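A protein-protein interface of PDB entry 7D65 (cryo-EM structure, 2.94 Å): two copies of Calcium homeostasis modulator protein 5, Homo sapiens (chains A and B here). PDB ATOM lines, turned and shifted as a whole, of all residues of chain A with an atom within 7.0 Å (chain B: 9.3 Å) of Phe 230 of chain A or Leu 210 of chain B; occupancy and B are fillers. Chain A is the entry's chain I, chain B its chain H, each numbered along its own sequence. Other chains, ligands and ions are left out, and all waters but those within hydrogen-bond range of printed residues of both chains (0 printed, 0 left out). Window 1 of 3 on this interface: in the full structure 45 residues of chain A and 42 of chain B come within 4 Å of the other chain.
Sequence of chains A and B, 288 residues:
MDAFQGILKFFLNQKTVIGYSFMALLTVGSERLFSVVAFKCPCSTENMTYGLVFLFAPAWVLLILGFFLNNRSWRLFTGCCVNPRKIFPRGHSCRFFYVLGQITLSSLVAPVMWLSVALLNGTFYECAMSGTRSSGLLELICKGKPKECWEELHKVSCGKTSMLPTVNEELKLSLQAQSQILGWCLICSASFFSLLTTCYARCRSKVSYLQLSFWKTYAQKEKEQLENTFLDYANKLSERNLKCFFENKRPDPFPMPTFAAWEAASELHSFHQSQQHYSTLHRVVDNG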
ATOM      1  N   THR A  78       2.343 -15.347   9.223  1.00  0.00           N
ATOM      2  CA  THR A  78       2.682 -16.737   8.950  1.00  0.00           C
ATOM      3  C   THR A  78       1.627 -17.377   8.060  1.00  0.00           C
ATOM      4  O   THR A  78       0.430 -17.279   8.332  1.00  0.00           O
ATOM      5  CB  THR A  78       2.813 -17.517  10.247  1.00  0.00           C
ATOM      6  OG1 THR A  78       3.624 -16.779  11.160  1.00  0.00           O
ATOM      7  CG2 THR A  78       3.465 -18.838   9.999  1.00  0.00           C
ATOM      8  N   GLN A 225      -4.302 -22.321  28.222  1.00  0.00           N
ATOM      9  CA  GLN A 225      -4.898 -23.619  27.940  1.00  0.00           C
ATOM     10  C   GLN A 225      -4.446 -24.162  26.598  1.00  0.00           C
ATOM     11  O   GLN A 225      -4.399 -25.379  26.410  1.00  0.00           O
ATOM     12  CB  GLN A 225      -6.417 -23.523  27.961  1.00  0.00           C
ATOM     13  CG  GLN A 225      -6.987 -22.795  29.138  1.00  0.00           C
ATOM     14  CD  GLN A 225      -7.179 -23.654  30.345  1.00  0.00           C
ATOM     15  OE1 GLN A 225      -6.549 -23.444  31.380  1.00  0.00           O
ATOM     16  NE2 GLN A 225      -8.066 -24.627  30.234  1.00  0.00           N
ATOM     17  N   LEU A 226      -4.118 -23.290  25.653  1.00  0.00           N
ATOM     18  CA  LEU A 226      -3.624 -23.742  24.364  1.00  0.00           C
ATOM     19  C   LEU A 226      -2.188 -24.221  24.428  1.00  0.00           C
ATOM     20  O   LEU A 226      -1.755 -24.941  23.534  1.00  0.00           O
ATOM     21  CB  LEU A 226      -3.735 -22.621  23.342  1.00  0.00           C
ATOM     22  CG  LEU A 226      -3.980 -22.964  21.887  1.00  0.00           C
ATOM     23  CD1 LEU A 226      -5.165 -23.876  21.767  1.00  0.00           C
ATOM     24  CD2 LEU A 226      -4.244 -21.692  21.160  1.00  0.00           C
ATOM     25  N   GLU A 227      -1.433 -23.829  25.446  1.00  0.00           N
ATOM     26  CA  GLU A 227      -0.106 -24.389  25.636  1.00  0.00           C
ATOM     27  C   GLU A 227      -0.127 -25.663  26.462  1.00  0.00           C
ATOM     28  O   GLU A 227       0.911 -26.310  26.597  1.00  0.00           O
ATOM     29  CB  GLU A 227       0.816 -23.362  26.287  1.00  0.00           C
ATOM     30  CG  GLU A 227       1.190 -22.221  25.361  1.00  0.00           C
ATOM     31  CD  GLU A 227       1.664 -20.976  26.098  1.00  0.00           C
ATOM     32  OE1 GLU A 227       1.823 -21.029  27.337  1.00  0.00           O
ATOM     33  OE2 GLU A 227       1.877 -19.939  25.436  1.00  0.00           O
ATOM     34  N   ASN A 228      -1.276 -26.038  27.013  1.00  0.00           N
ATOM     35  CA  ASN A 228      -1.415 -27.285  27.745  1.00  0.00           C
ATOM     36  C   ASN A 228      -2.161 -28.350  26.966  1.00  0.00           C
ATOM     37  O   ASN A 228      -2.069 -29.525  27.321  1.00  0.00           O
ATOM     38  CB  ASN A 228      -2.146 -27.054  29.067  1.00  0.00           C
ATOM     39  CG  ASN A 228      -1.275 -26.403  30.098  1.00  0.00           C
ATOM     40  OD1 ASN A 228      -0.055 -26.407  29.984  1.00  0.00           O
ATOM     41  ND2 ASN A 228      -1.895 -25.835  31.118  1.00  0.00           N
ATOM     42  N   THR A 229      -2.918 -27.968  25.941  1.00  0.00           N
ATOM     43  CA  THR A 229      -3.532 -28.953  25.065  1.00  0.00           C
ATOM     44  C   THR A 229      -2.562 -29.376  23.978  1.00  0.00           C
ATOM     45  O   THR A 229      -2.536 -30.547  23.591  1.00  0.00           O
ATOM     46  CB  THR A 229      -4.822 -28.388  24.475  1.00  0.00           C
ATOM     47  OG1 THR A 229      -5.681 -27.993  25.545  1.00  0.00           O
ATOM     48  CG2 THR A 229      -5.555 -29.410  23.652  1.00  0.00           C
ATOM     49  N   PHE A 230      -1.729 -28.449  23.501  1.00  0.00           N
ATOM     50  CA  PHE A 230      -0.697 -28.797  22.529  1.00  0.00           C
ATOM     51  C   PHE A 230       0.340 -29.726  23.127  1.00  0.00           C
ATOM     52  O   PHE A 230       0.948 -30.511  22.403  1.00  0.00           O
ATOM     53  CB  PHE A 230       0.007 -27.548  22.010  1.00  0.00           C
ATOM     54  CG  PHE A 230      -0.790 -26.755  21.030  1.00  0.00           C
ATOM     55  CD1 PHE A 230      -1.943 -27.259  20.468  1.00  0.00           C
ATOM     56  CD2 PHE A 230      -0.378 -25.497  20.669  1.00  0.00           C
ATOM     57  CE1 PHE A 230      -2.663 -26.519  19.574  1.00  0.00           C
ATOM     58  CE2 PHE A 230      -1.095 -24.760  19.776  1.00  0.00           C
ATOM     59  CZ  PHE A 230      -2.238 -25.273  19.228  1.00  0.00           C
ATOM     60  N   LEU A 231       0.558 -29.648  24.430  1.00  0.00           N
ATOM     61  CA  LEU A 231       1.533 -30.469  25.120  1.00  0.00           C
ATOM     62  C   LEU A 231       0.924 -31.759  25.646  1.00  0.00           C
ATOM     63  O   LEU A 231       1.656 -32.660  26.049  1.00  0.00           O
ATOM     64  CB  LEU A 231       2.151 -29.641  26.245  1.00  0.00           C
ATOM     65  CG  LEU A 231       3.399 -30.018  27.019  1.00  0.00           C
ATOM     66  CD1 LEU A 231       4.152 -28.750  27.311  1.00  0.00           C
ATOM     67  CD2 LEU A 231       3.024 -30.684  28.312  1.00  0.00           C
ATOM     68  N   ASP A 232      -0.395 -31.866  25.630  1.00  0.00           N
ATOM     69  CA  ASP A 232      -1.109 -33.079  25.995  1.00  0.00           C
ATOM     70  C   ASP A 232      -1.369 -33.975  24.796  1.00  0.00           C
ATOM     71  O   ASP A 232      -1.424 -35.199  24.943  1.00  0.00           O
ATOM     72  CB  ASP A 232      -2.435 -32.696  26.656  1.00  0.00           C
ATOM     73  CG  ASP A 232      -3.146 -33.865  27.260  1.00  0.00           C
ATOM     74  OD1 ASP A 232      -2.516 -34.582  28.058  1.00  0.00           O
ATOM     75  OD2 ASP A 232      -4.342 -34.060  26.948  1.00  0.00           O
ATOM     76  N   TYR A 233      -1.536 -33.392  23.615  1.00  0.00           N
ATOM     77  CA  TYR A 233      -1.734 -34.132  22.382  1.00  0.00           C
ATOM     78  C   TYR A 233      -0.432 -34.427  21.661  1.00  0.00           C
ATOM     79  O   TYR A 233      -0.450 -35.147  20.661  1.00  0.00           O
ATOM     80  CB  TYR A 233      -2.658 -33.363  21.444  1.00  0.00           C
ATOM     81  CG  TYR A 233      -4.121 -33.599  21.683  1.00  0.00           C
ATOM     82  CD1 TYR A 233      -4.893 -34.265  20.751  1.00  0.00           C
ATOM     83  CD2 TYR A 233      -4.731 -33.147  22.833  1.00  0.00           C
ATOM     84  CE1 TYR A 233      -6.232 -34.480  20.962  1.00  0.00           C
ATOM     85  CE2 TYR A 233      -6.067 -33.355  23.057  1.00  0.00           C
ATOM     86  CZ  TYR A 233      -6.813 -34.020  22.121  1.00  0.00           C
ATOM     87  OH  TYR A 233      -8.154 -34.225  22.348  1.00  0.00           O
ATOM     88  N   ALA A 234       0.688 -33.879  22.121  1.00  0.00           N
ATOM     89  CA  ALA A 234       1.989 -34.220  21.568  1.00  0.00           C
ATOM     90  C   ALA A 234       2.702 -35.292  22.364  1.00  0.00           C
ATOM     91  O   ALA A 234       3.546 -35.994  21.807  1.00  0.00           O
ATOM     92  CB  ALA A 234       2.886 -32.985  21.494  1.00  0.00           C
ATOM     93  N   ASN A 235       2.397 -35.424  23.650  1.00  0.00           N
ATOM     94  CA  ASN A 235       2.873 -36.573  24.402  1.00  0.00           C
ATOM     95  C   ASN A 235       2.129 -37.833  23.996  1.00  0.00           C
ATOM     96  O   ASN A 235       2.697 -38.925  24.008  1.00  0.00           O
ATOM     97  CB  ASN A 235       2.716 -36.324  25.896  1.00  0.00           C
ATOM     98  CG  ASN A 235       4.013 -35.957  26.558  1.00  0.00           C
ATOM     99  OD1 ASN A 235       5.068 -36.466  26.198  1.00  0.00           O
ATOM    100  ND2 ASN A 235       3.946 -35.072  27.541  1.00  0.00           N
ATOM    101  N   ALA A 261      -9.803 -26.632   9.067  1.00  0.00           N
ATOM    102  CA  ALA A 261     -10.171 -26.051  10.348  1.00  0.00           C
ATOM    103  C   ALA A 261      -8.982 -25.512  11.123  1.00  0.00           C
ATOM    104  O   ALA A 261      -9.177 -24.741  12.063  1.00  0.00           O
ATOM    105  CB  ALA A 261     -10.900 -27.076  11.210  1.00  0.00           C
ATOM    106  N   TRP A 262      -7.762 -25.919  10.773  1.00  0.00           N
ATOM    107  CA  TRP A 262      -6.582 -25.279  11.333  1.00  0.00           C
ATOM    108  C   TRP A 262      -6.397 -23.885  10.760  1.00  0.00           C
ATOM    109  O   TRP A 262      -5.854 -23.006  11.432  1.00  0.00           O
ATOM    110  CB  TRP A 262      -5.333 -26.106  11.042  1.00  0.00           C
ATOM    111  CG  TRP A 262      -5.000 -27.249  11.969  1.00  0.00           C
ATOM    112  CD1 TRP A 262      -5.037 -28.566  11.666  1.00  0.00           C
ATOM    113  CD2 TRP A 262      -4.507 -27.164  13.308  1.00  0.00           C
ATOM    114  NE1 TRP A 262      -4.632 -29.312  12.731  1.00  0.00           N
ATOM    115  CE2 TRP A 262      -4.297 -28.474  13.755  1.00  0.00           C
ATOM    116  CE3 TRP A 262      -4.235 -26.109  14.176  1.00  0.00           C
ATOM    117  CZ2 TRP A 262      -3.832 -28.759  15.027  1.00  0.00           C
ATOM    118  CZ3 TRP A 262      -3.772 -26.397  15.437  1.00  0.00           C
ATOM    119  CH2 TRP A 262      -3.575 -27.707  15.851  1.00  0.00           C
ATOM    120  N   ALA A 265      -9.248 -21.135  12.270  1.00  0.00           N
ATOM    121  CA  ALA A 265      -8.999 -20.654  13.619  1.00  0.00           C
ATOM    122  C   ALA A 265      -7.713 -19.853  13.736  1.00  0.00           C
ATOM    123  O   ALA A 265      -7.217 -19.661  14.848  1.00  0.00           O
ATOM    124  CB  ALA A 265      -8.961 -21.822  14.597  1.00  0.00           C
ATOM    125  N   SER A 266      -7.165 -19.387  12.617  1.00  0.00           N
ATOM    126  CA  SER A 266      -5.953 -18.580  12.590  1.00  0.00           C
ATOM    127  C   SER A 266      -6.164 -17.269  11.853  1.00  0.00           C
ATOM    128  O   SER A 266      -5.199 -16.668  11.384  1.00  0.00           O
ATOM    129  CB  SER A 266      -4.807 -19.350  11.940  1.00  0.00           C
ATOM    130  OG  SER A 266      -4.181 -20.218  12.857  1.00  0.00           O
ATOM    131  N   LEU A 281     -11.290 -18.424  17.654  1.00  0.00           N
ATOM    132  CA  LEU A 281     -11.564 -19.809  17.995  1.00  0.00           C
ATOM    133  C   LEU A 281     -12.906 -19.976  18.681  1.00  0.00           C
ATOM    134  O   LEU A 281     -13.496 -21.054  18.608  1.00  0.00           O
ATOM    135  CB  LEU A 281     -10.459 -20.349  18.902  1.00  0.00           C
ATOM    136  CG  LEU A 281     -10.381 -21.841  19.191  1.00  0.00           C
ATOM    137  CD1 LEU A 281     -10.617 -22.609  17.936  1.00  0.00           C
ATOM    138  CD2 LEU A 281      -9.032 -22.169  19.731  1.00  0.00           C
ATOM    139  N   ARG B 202       8.591 -17.131   6.685  1.00  0.00           N
ATOM    140  CA  ARG B 202       7.302 -17.287   7.342  1.00  0.00           C
ATOM    141  C   ARG B 202       6.138 -16.961   6.424  1.00  0.00           C
ATOM    142  O   ARG B 202       5.091 -17.601   6.522  1.00  0.00           O
ATOM    143  CB  ARG B 202       7.216 -16.398   8.580  1.00  0.00           C
ATOM    144  CG  ARG B 202       8.271 -16.672   9.618  1.00  0.00           C
ATOM    145  CD  ARG B 202       8.063 -18.016  10.254  1.00  0.00           C
ATOM    146  NE  ARG B 202       7.094 -17.953  11.338  1.00  0.00           N
ATOM    147  CZ  ARG B 202       7.402 -18.105  12.619  1.00  0.00           C
ATOM    148  NH1 ARG B 202       8.657 -18.327  12.974  1.00  0.00           N
ATOM    149  NH2 ARG B 202       6.458 -18.038  13.545  1.00  0.00           N
ATOM    150  N   SER B 205       5.324 -20.071   4.299  1.00  0.00           N
ATOM    151  CA  SER B 205       5.182 -21.324   5.011  1.00  0.00           C
ATOM    152  C   SER B 205       3.959 -22.075   4.505  1.00  0.00           C
ATOM    153  O   SER B 205       3.090 -21.516   3.835  1.00  0.00           O
ATOM    154  CB  SER B 205       5.070 -21.065   6.509  1.00  0.00           C
ATOM    155  OG  SER B 205       4.644 -22.210   7.205  1.00  0.00           O
ATOM    156  N   VAL B 207       1.900 -23.930   6.606  1.00  0.00           N
ATOM    157  CA  VAL B 207       0.897 -23.995   7.654  1.00  0.00           C
ATOM    158  C   VAL B 207       0.715 -22.602   8.238  1.00  0.00           C
ATOM    159  O   VAL B 207       1.576 -21.733   8.112  1.00  0.00           O
ATOM    160  CB  VAL B 207       1.295 -24.998   8.749  1.00  0.00           C
ATOM    161  CG1 VAL B 207       1.245 -26.385   8.207  1.00  0.00           C
ATOM    162  CG2 VAL B 207       2.683 -24.703   9.242  1.00  0.00           C
ATOM    163  N   SER B 208      -0.414 -22.401   8.905  1.00  0.00           N
ATOM    164  CA  SER B 208      -0.717 -21.126   9.538  1.00  0.00           C
ATOM    165  C   SER B 208      -0.008 -21.047  10.883  1.00  0.00           C
ATOM    166  O   SER B 208       0.842 -21.873  11.206  1.00  0.00           O
ATOM    167  CB  SER B 208      -2.219 -20.953   9.669  1.00  0.00           C
ATOM    168  OG  SER B 208      -2.781 -20.608   8.421  1.00  0.00           O
ATOM    169  N   TYR B 209      -0.346 -20.047  11.692  1.00  0.00           N
ATOM    170  CA  TYR B 209       0.418 -19.817  12.912  1.00  0.00           C
ATOM    171  C   TYR B 209       0.109 -20.852  13.980  1.00  0.00           C
ATOM    172  O   TYR B 209       0.997 -21.252  14.736  1.00  0.00           O
ATOM    173  CB  TYR B 209       0.151 -18.420  13.457  1.00  0.00           C
ATOM    174  CG  TYR B 209       0.850 -18.197  14.769  1.00  0.00           C
ATOM    175  CD1 TYR B 209       2.232 -18.092  14.822  1.00  0.00           C
ATOM    176  CD2 TYR B 209       0.142 -18.129  15.963  1.00  0.00           C
ATOM    177  CE1 TYR B 209       2.891 -17.908  16.014  1.00  0.00           C
ATOM    178  CE2 TYR B 209       0.795 -17.953  17.164  1.00  0.00           C
ATOM    179  CZ  TYR B 209       2.169 -17.835  17.180  1.00  0.00           C
ATOM    180  OH  TYR B 209       2.824 -17.649  18.370  1.00  0.00           O
ATOM    181  N   LEU B 210      -1.137 -21.293  14.069  1.00  0.00           N
ATOM    182  CA  LEU B 210      -1.527 -22.183  15.152  1.00  0.00           C
ATOM    183  C   LEU B 210      -1.040 -23.605  14.907  1.00  0.00           C
ATOM    184  O   LEU B 210      -0.674 -24.307  15.850  1.00  0.00           O
ATOM    185  CB  LEU B 210      -3.042 -22.145  15.312  1.00  0.00           C
ATOM    186  CG  LEU B 210      -3.631 -22.375  16.688  1.00  0.00           C
ATOM    187  CD1 LEU B 210      -3.156 -21.305  17.603  1.00  0.00           C
ATOM    188  CD2 LEU B 210      -5.118 -22.331  16.573  1.00  0.00           C
ATOM    189  N   GLN B 211      -1.015 -24.036  13.649  1.00  0.00           N
ATOM    190  CA  GLN B 211      -0.494 -25.354  13.324  1.00  0.00           C
ATOM    191  C   GLN B 211       1.019 -25.406  13.430  1.00  0.00           C
ATOM    192  O   GLN B 211       1.576 -26.454  13.758  1.00  0.00           O
ATOM    193  CB  GLN B 211      -0.929 -25.755  11.926  1.00  0.00           C
ATOM    194  CG  GLN B 211      -0.784 -27.214  11.650  1.00  0.00           C
ATOM    195  CD  GLN B 211      -1.516 -27.626  10.421  1.00  0.00           C
ATOM    196  OE1 GLN B 211      -2.144 -26.810   9.761  1.00  0.00           O
ATOM    197  NE2 GLN B 211      -1.445 -28.899  10.097  1.00  0.00           N
ATOM    198  N   LEU B 212       1.702 -24.299  13.165  1.00  0.00           N
ATOM    199  CA  LEU B 212       3.146 -24.259  13.337  1.00  0.00           C
ATOM    200  C   LEU B 212       3.551 -24.260  14.801  1.00  0.00           C
ATOM    201  O   LEU B 212       4.708 -24.538  15.111  1.00  0.00           O
ATOM    202  CB  LEU B 212       3.720 -23.032  12.638  1.00  0.00           C
ATOM    203  CG  LEU B 212       5.212 -22.967  12.342  1.00  0.00           C
ATOM    204  CD1 LEU B 212       5.627 -24.109  11.477  1.00  0.00           C
ATOM    205  CD2 LEU B 212       5.531 -21.671  11.678  1.00  0.00           C
ATOM    206  N   SER B 213       2.634 -23.972  15.706  1.00  0.00           N
ATOM    207  CA  SER B 213       2.943 -23.998  17.120  1.00  0.00           C
ATOM    208  C   SER B 213       2.710 -25.361  17.746  1.00  0.00           C
ATOM    209  O   SER B 213       3.258 -25.636  18.815  1.00  0.00           O
ATOM    210  CB  SER B 213       2.113 -22.945  17.844  1.00  0.00           C
ATOM    211  OG  SER B 213       2.447 -22.898  19.210  1.00  0.00           O
ATOM    212  N   PHE B 214       1.902 -26.210  17.117  1.00  0.00           N
ATOM    213  CA  PHE B 214       1.782 -27.597  17.540  1.00  0.00           C
ATOM    214  C   PHE B 214       2.896 -28.443  16.956  1.00  0.00           C
ATOM    215  O   PHE B 214       3.356 -29.382  17.602  1.00  0.00           O
ATOM    216  CB  PHE B 214       0.428 -28.162  17.123  1.00  0.00           C
ATOM    217  CG  PHE B 214       0.303 -29.638  17.317  1.00  0.00           C
ATOM    218  CD1 PHE B 214       0.314 -30.184  18.582  1.00  0.00           C
ATOM    219  CD2 PHE B 214       0.179 -30.480  16.236  1.00  0.00           C
ATOM    220  CE1 PHE B 214       0.205 -31.536  18.760  1.00  0.00           C
ATOM    221  CE2 PHE B 214       0.075 -31.827  16.416  1.00  0.00           C
ATOM    222  CZ  PHE B 214       0.083 -32.356  17.677  1.00  0.00           C
ATOM    223  N   TRP B 215       3.338 -28.101  15.747  1.00  0.00           N
ATOM    224  CA  TRP B 215       4.456 -28.776  15.102  1.00  0.00           C
ATOM    225  C   TRP B 215       5.750 -28.603  15.888  1.00  0.00           C
ATOM    226  O   TRP B 215       6.572 -29.518  15.944  1.00  0.00           O
ATOM    227  CB  TRP B 215       4.585 -28.231  13.681  1.00  0.00           C
ATOM    228  CG  TRP B 215       5.466 -28.954  12.726  1.00  0.00           C
ATOM    229  CD1 TRP B 215       6.240 -30.037  12.970  1.00  0.00           C
ATOM    230  CD2 TRP B 215       5.666 -28.626  11.348  1.00  0.00           C
ATOM    231  NE1 TRP B 215       6.916 -30.403  11.841  1.00  0.00           N
ATOM    232  CE2 TRP B 215       6.576 -29.551  10.828  1.00  0.00           C
ATOM    233  CE3 TRP B 215       5.159 -27.639  10.507  1.00  0.00           C
ATOM    234  CZ2 TRP B 215       6.989 -29.521   9.506  1.00  0.00           C
ATOM    235  CZ3 TRP B 215       5.573 -27.610   9.198  1.00  0.00           C
ATOM    236  CH2 TRP B 215       6.477 -28.541   8.710  1.00  0.00           C
ATOM    237  N   LYS B 216       5.947 -27.453  16.524  1.00  0.00           N
ATOM    238  CA  LYS B 216       7.168 -27.244  17.293  1.00  0.00           C
ATOM    239  C   LYS B 216       7.106 -27.871  18.677  1.00  0.00           C
ATOM    240  O   LYS B 216       8.150 -28.189  19.246  1.00  0.00           O
ATOM    241  CB  LYS B 216       7.457 -25.756  17.434  1.00  0.00           C
ATOM    242  CG  LYS B 216       8.106 -25.132  16.237  1.00  0.00           C
ATOM    243  CD  LYS B 216       8.260 -23.643  16.440  1.00  0.00           C
ATOM    244  CE  LYS B 216       8.733 -22.951  15.176  1.00  0.00           C
ATOM    245  NZ  LYS B 216       9.592 -23.827  14.344  1.00  0.00           N
ATOM    246  N   THR B 217       5.917 -28.024  19.252  1.00  0.00           N
ATOM    247  CA  THR B 217       5.801 -28.752  20.508  1.00  0.00           C
ATOM    248  C   THR B 217       5.976 -30.242  20.290  1.00  0.00           C
ATOM    249  O   THR B 217       6.489 -30.940  21.168  1.00  0.00           O
ATOM    250  CB  THR B 217       4.446 -28.478  21.150  1.00  0.00           C
ATOM    251  OG1 THR B 217       4.152 -27.085  21.051  1.00  0.00           O
ATOM    252  CG2 THR B 217       4.441 -28.868  22.606  1.00  0.00           C
ATOM    253  N   TYR B 218       5.557 -30.742  19.130  1.00  0.00           N
ATOM    254  CA  TYR B 218       5.710 -32.157  18.836  1.00  0.00           C
ATOM    255  C   TYR B 218       7.165 -32.513  18.606  1.00  0.00           C
ATOM    256  O   TYR B 218       7.651 -33.508  19.142  1.00  0.00           O
ATOM    257  CB  TYR B 218       4.874 -32.534  17.622  1.00  0.00           C
ATOM    258  CG  TYR B 218       5.137 -33.931  17.148  1.00  0.00           C
ATOM    259  CD1 TYR B 218       4.695 -35.014  17.872  1.00  0.00           C
ATOM    260  CD2 TYR B 218       5.840 -34.168  15.984  1.00  0.00           C
ATOM    261  CE1 TYR B 218       4.944 -36.289  17.453  1.00  0.00           C
ATOM    262  CE2 TYR B 218       6.090 -35.443  15.561  1.00  0.00           C
ATOM    263  CZ  TYR B 218       5.637 -36.498  16.297  1.00  0.00           C
ATOM    264  OH  TYR B 218       5.885 -37.779  15.879  1.00  0.00           O
ATOM    265  N   ALA B 219       7.880 -31.704  17.832  1.00  0.00           N
ATOM    266  CA  ALA B 219       9.254 -32.028  17.475  1.00  0.00           C
ATOM    267  C   ALA B 219      10.207 -31.913  18.646  1.00  0.00           C
ATOM    268  O   ALA B 219      11.285 -32.505  18.605  1.00  0.00           O
ATOM    269  CB  ALA B 219       9.730 -31.129  16.343  1.00  0.00           C
ATOM    270  N   LYS B 221       9.245 -32.902  21.750  1.00  0.00           N
ATOM    271  CA  LYS B 221       8.918 -34.042  22.583  1.00  0.00           C
ATOM    272  C   LYS B 221       9.002 -35.360  21.844  1.00  0.00           C
ATOM    273  O   LYS B 221       8.639 -36.384  22.408  1.00  0.00           O
ATOM    274  CB  LYS B 221       7.530 -33.871  23.181  1.00  0.00           C
ATOM    275  CG  LYS B 221       7.555 -32.983  24.393  1.00  0.00           C
ATOM    276  CD  LYS B 221       6.352 -33.199  25.239  1.00  0.00           C
ATOM    277  CE  LYS B 221       5.133 -32.777  24.484  1.00  0.00           C
ATOM    278  NZ  LYS B 221       3.918 -32.959  25.307  1.00  0.00           N
ATOM    279  N   TYR B 278       3.886 -34.698  10.837  1.00  0.00           N
ATOM    280  CA  TYR B 278       4.723 -33.755  11.555  1.00  0.00           C
ATOM    281  C   TYR B 278       6.158 -34.222  11.718  1.00  0.00           C
ATOM    282  O   TYR B 278       6.970 -33.482  12.274  1.00  0.00           O
ATOM    283  CB  TYR B 278       4.110 -33.462  12.922  1.00  0.00           C
ATOM    284  CG  TYR B 278       2.742 -32.844  12.815  1.00  0.00           C
ATOM    285  CD1 TYR B 278       2.584 -31.532  12.396  1.00  0.00           C
ATOM    286  CD2 TYR B 278       1.611 -33.574  13.113  1.00  0.00           C
ATOM    287  CE1 TYR B 278       1.341 -30.970  12.284  1.00  0.00           C
ATOM    288  CE2 TYR B 278       0.362 -33.012  13.005  1.00  0.00           C
ATOM    289  CZ  TYR B 278       0.236 -31.714  12.590  1.00  0.00           C
ATOM    290  OH  TYR B 278      -1.005 -31.158  12.481  1.00  0.00           O
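N of Leu 210 of chain B sits close to OG of Ser 266 of chain A, 3.4 Å away. The side-chain amide nitrogen of Asn 235 of chain A lies close to the side-chain amino group of Lys 221 of chain B, at 3.1 Å. The backbone carbonyl oxygen of Leu 231 of chain A lies close to the side-chain amino group of Lys 221 of chain B (2.4 Å).
OG of Ser 205 of chain B lies within hydrogen-bond range of O of Val 207 of chain B (3.2 Å). The side-chain amide nitrogen of Gln 211 of chain B lies within hydrogen-bond range of the side-chain hydroxyl of Tyr 278 of chain B, 3.3 Å away. The backbone carbonyl oxygen (O) of Ser 213 of chain B lies within hydrogen-bond range of the side-chain hydroxyl (OG1) of Thr 217 of chain B, at 2.8 Å.
Among the printed residues, merely in contact across the chains: Trp 262 of chain A with Gln 211 of chain B (3.5 Å), Thr 78 of chain A with Arg 202 of chain B (3.5 Å), Leu 226 of chain A with Leu 210 of chain B (3.7 Å), Ala 234 of chain A with Lys 221 of chain B (3.7 Å), Trp 262 of chain A with Leu 210 of chain B (3.8 Å), Ser 266 of chain A with Ser 208 of chain B (3.8 Å), Ala 265 of chain A with Leu 210 of chain B (3.8 Å), Phe 230 of chain A with Leu 210 of chain B (3.8 Å), Phe 230 of chain A with Phe 214 of chain B (3.9 Å), Phe 230 of chain A with Thr 217 of chain B (3.9 Å), Thr 78 of chain A with Leu 212 of chain B (3.9 Å), Thr 78 of chain A with Val 207 of chain B (3.9 Å) and Ala 234 of chain A with Tyr 218 of chain B (3.97 Å).
Printed residues of chain B within 4 Å of Thr 78 of chain A: Arg 202, Val 207 and Leu 212. Glu 227 of chain A touches none of the printed residues of chain B. Of chain B, only Leu 210, Phe 214 and Thr 217 come within 4 Å of Phe 230 of chain A. Tyr 233 of chain A touches none of the printed residues of chain B. Of the printed residues of chain B, Asn 235 of chain A touches Lys 221 (3.1 Å). Printed residues of chain B within 4 Å of Trp 262 of chain A: Leu 210 and Gln 211. The nearest printed residue of chain B that does not touch Asn 235 of chain A is Tyr 218 of chain B (6.2 Å).
Printed residues of chain A that touch a printed residue of chain B: Thr 78, Leu 226, Phe 230, Leu 231, Ala 234, Asn 235, Trp 262, Ala 265 and Ser 266. Hydrophobic or aromatic side chains of chain A that line the printed part of chain B: Leu 226, Phe 230, Leu 231, Ala 234 and Trp 262. Printed residues of chain B that touch a printed residue of chain A: Arg 202, Val 207, Ser 208, Leu 210, Gln 211, Leu 212, Phe 214, Thr 217, Tyr 218 and Lys 221. Along chain B the printed residues that touch a printed residue of chain A span positions 202 to 221. Among the printed residues, no Asp or Glu carboxylate lies within 4 Å of a Lys or Arg side-chain nitrogen of the other chain.
No position is printed for both chains.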
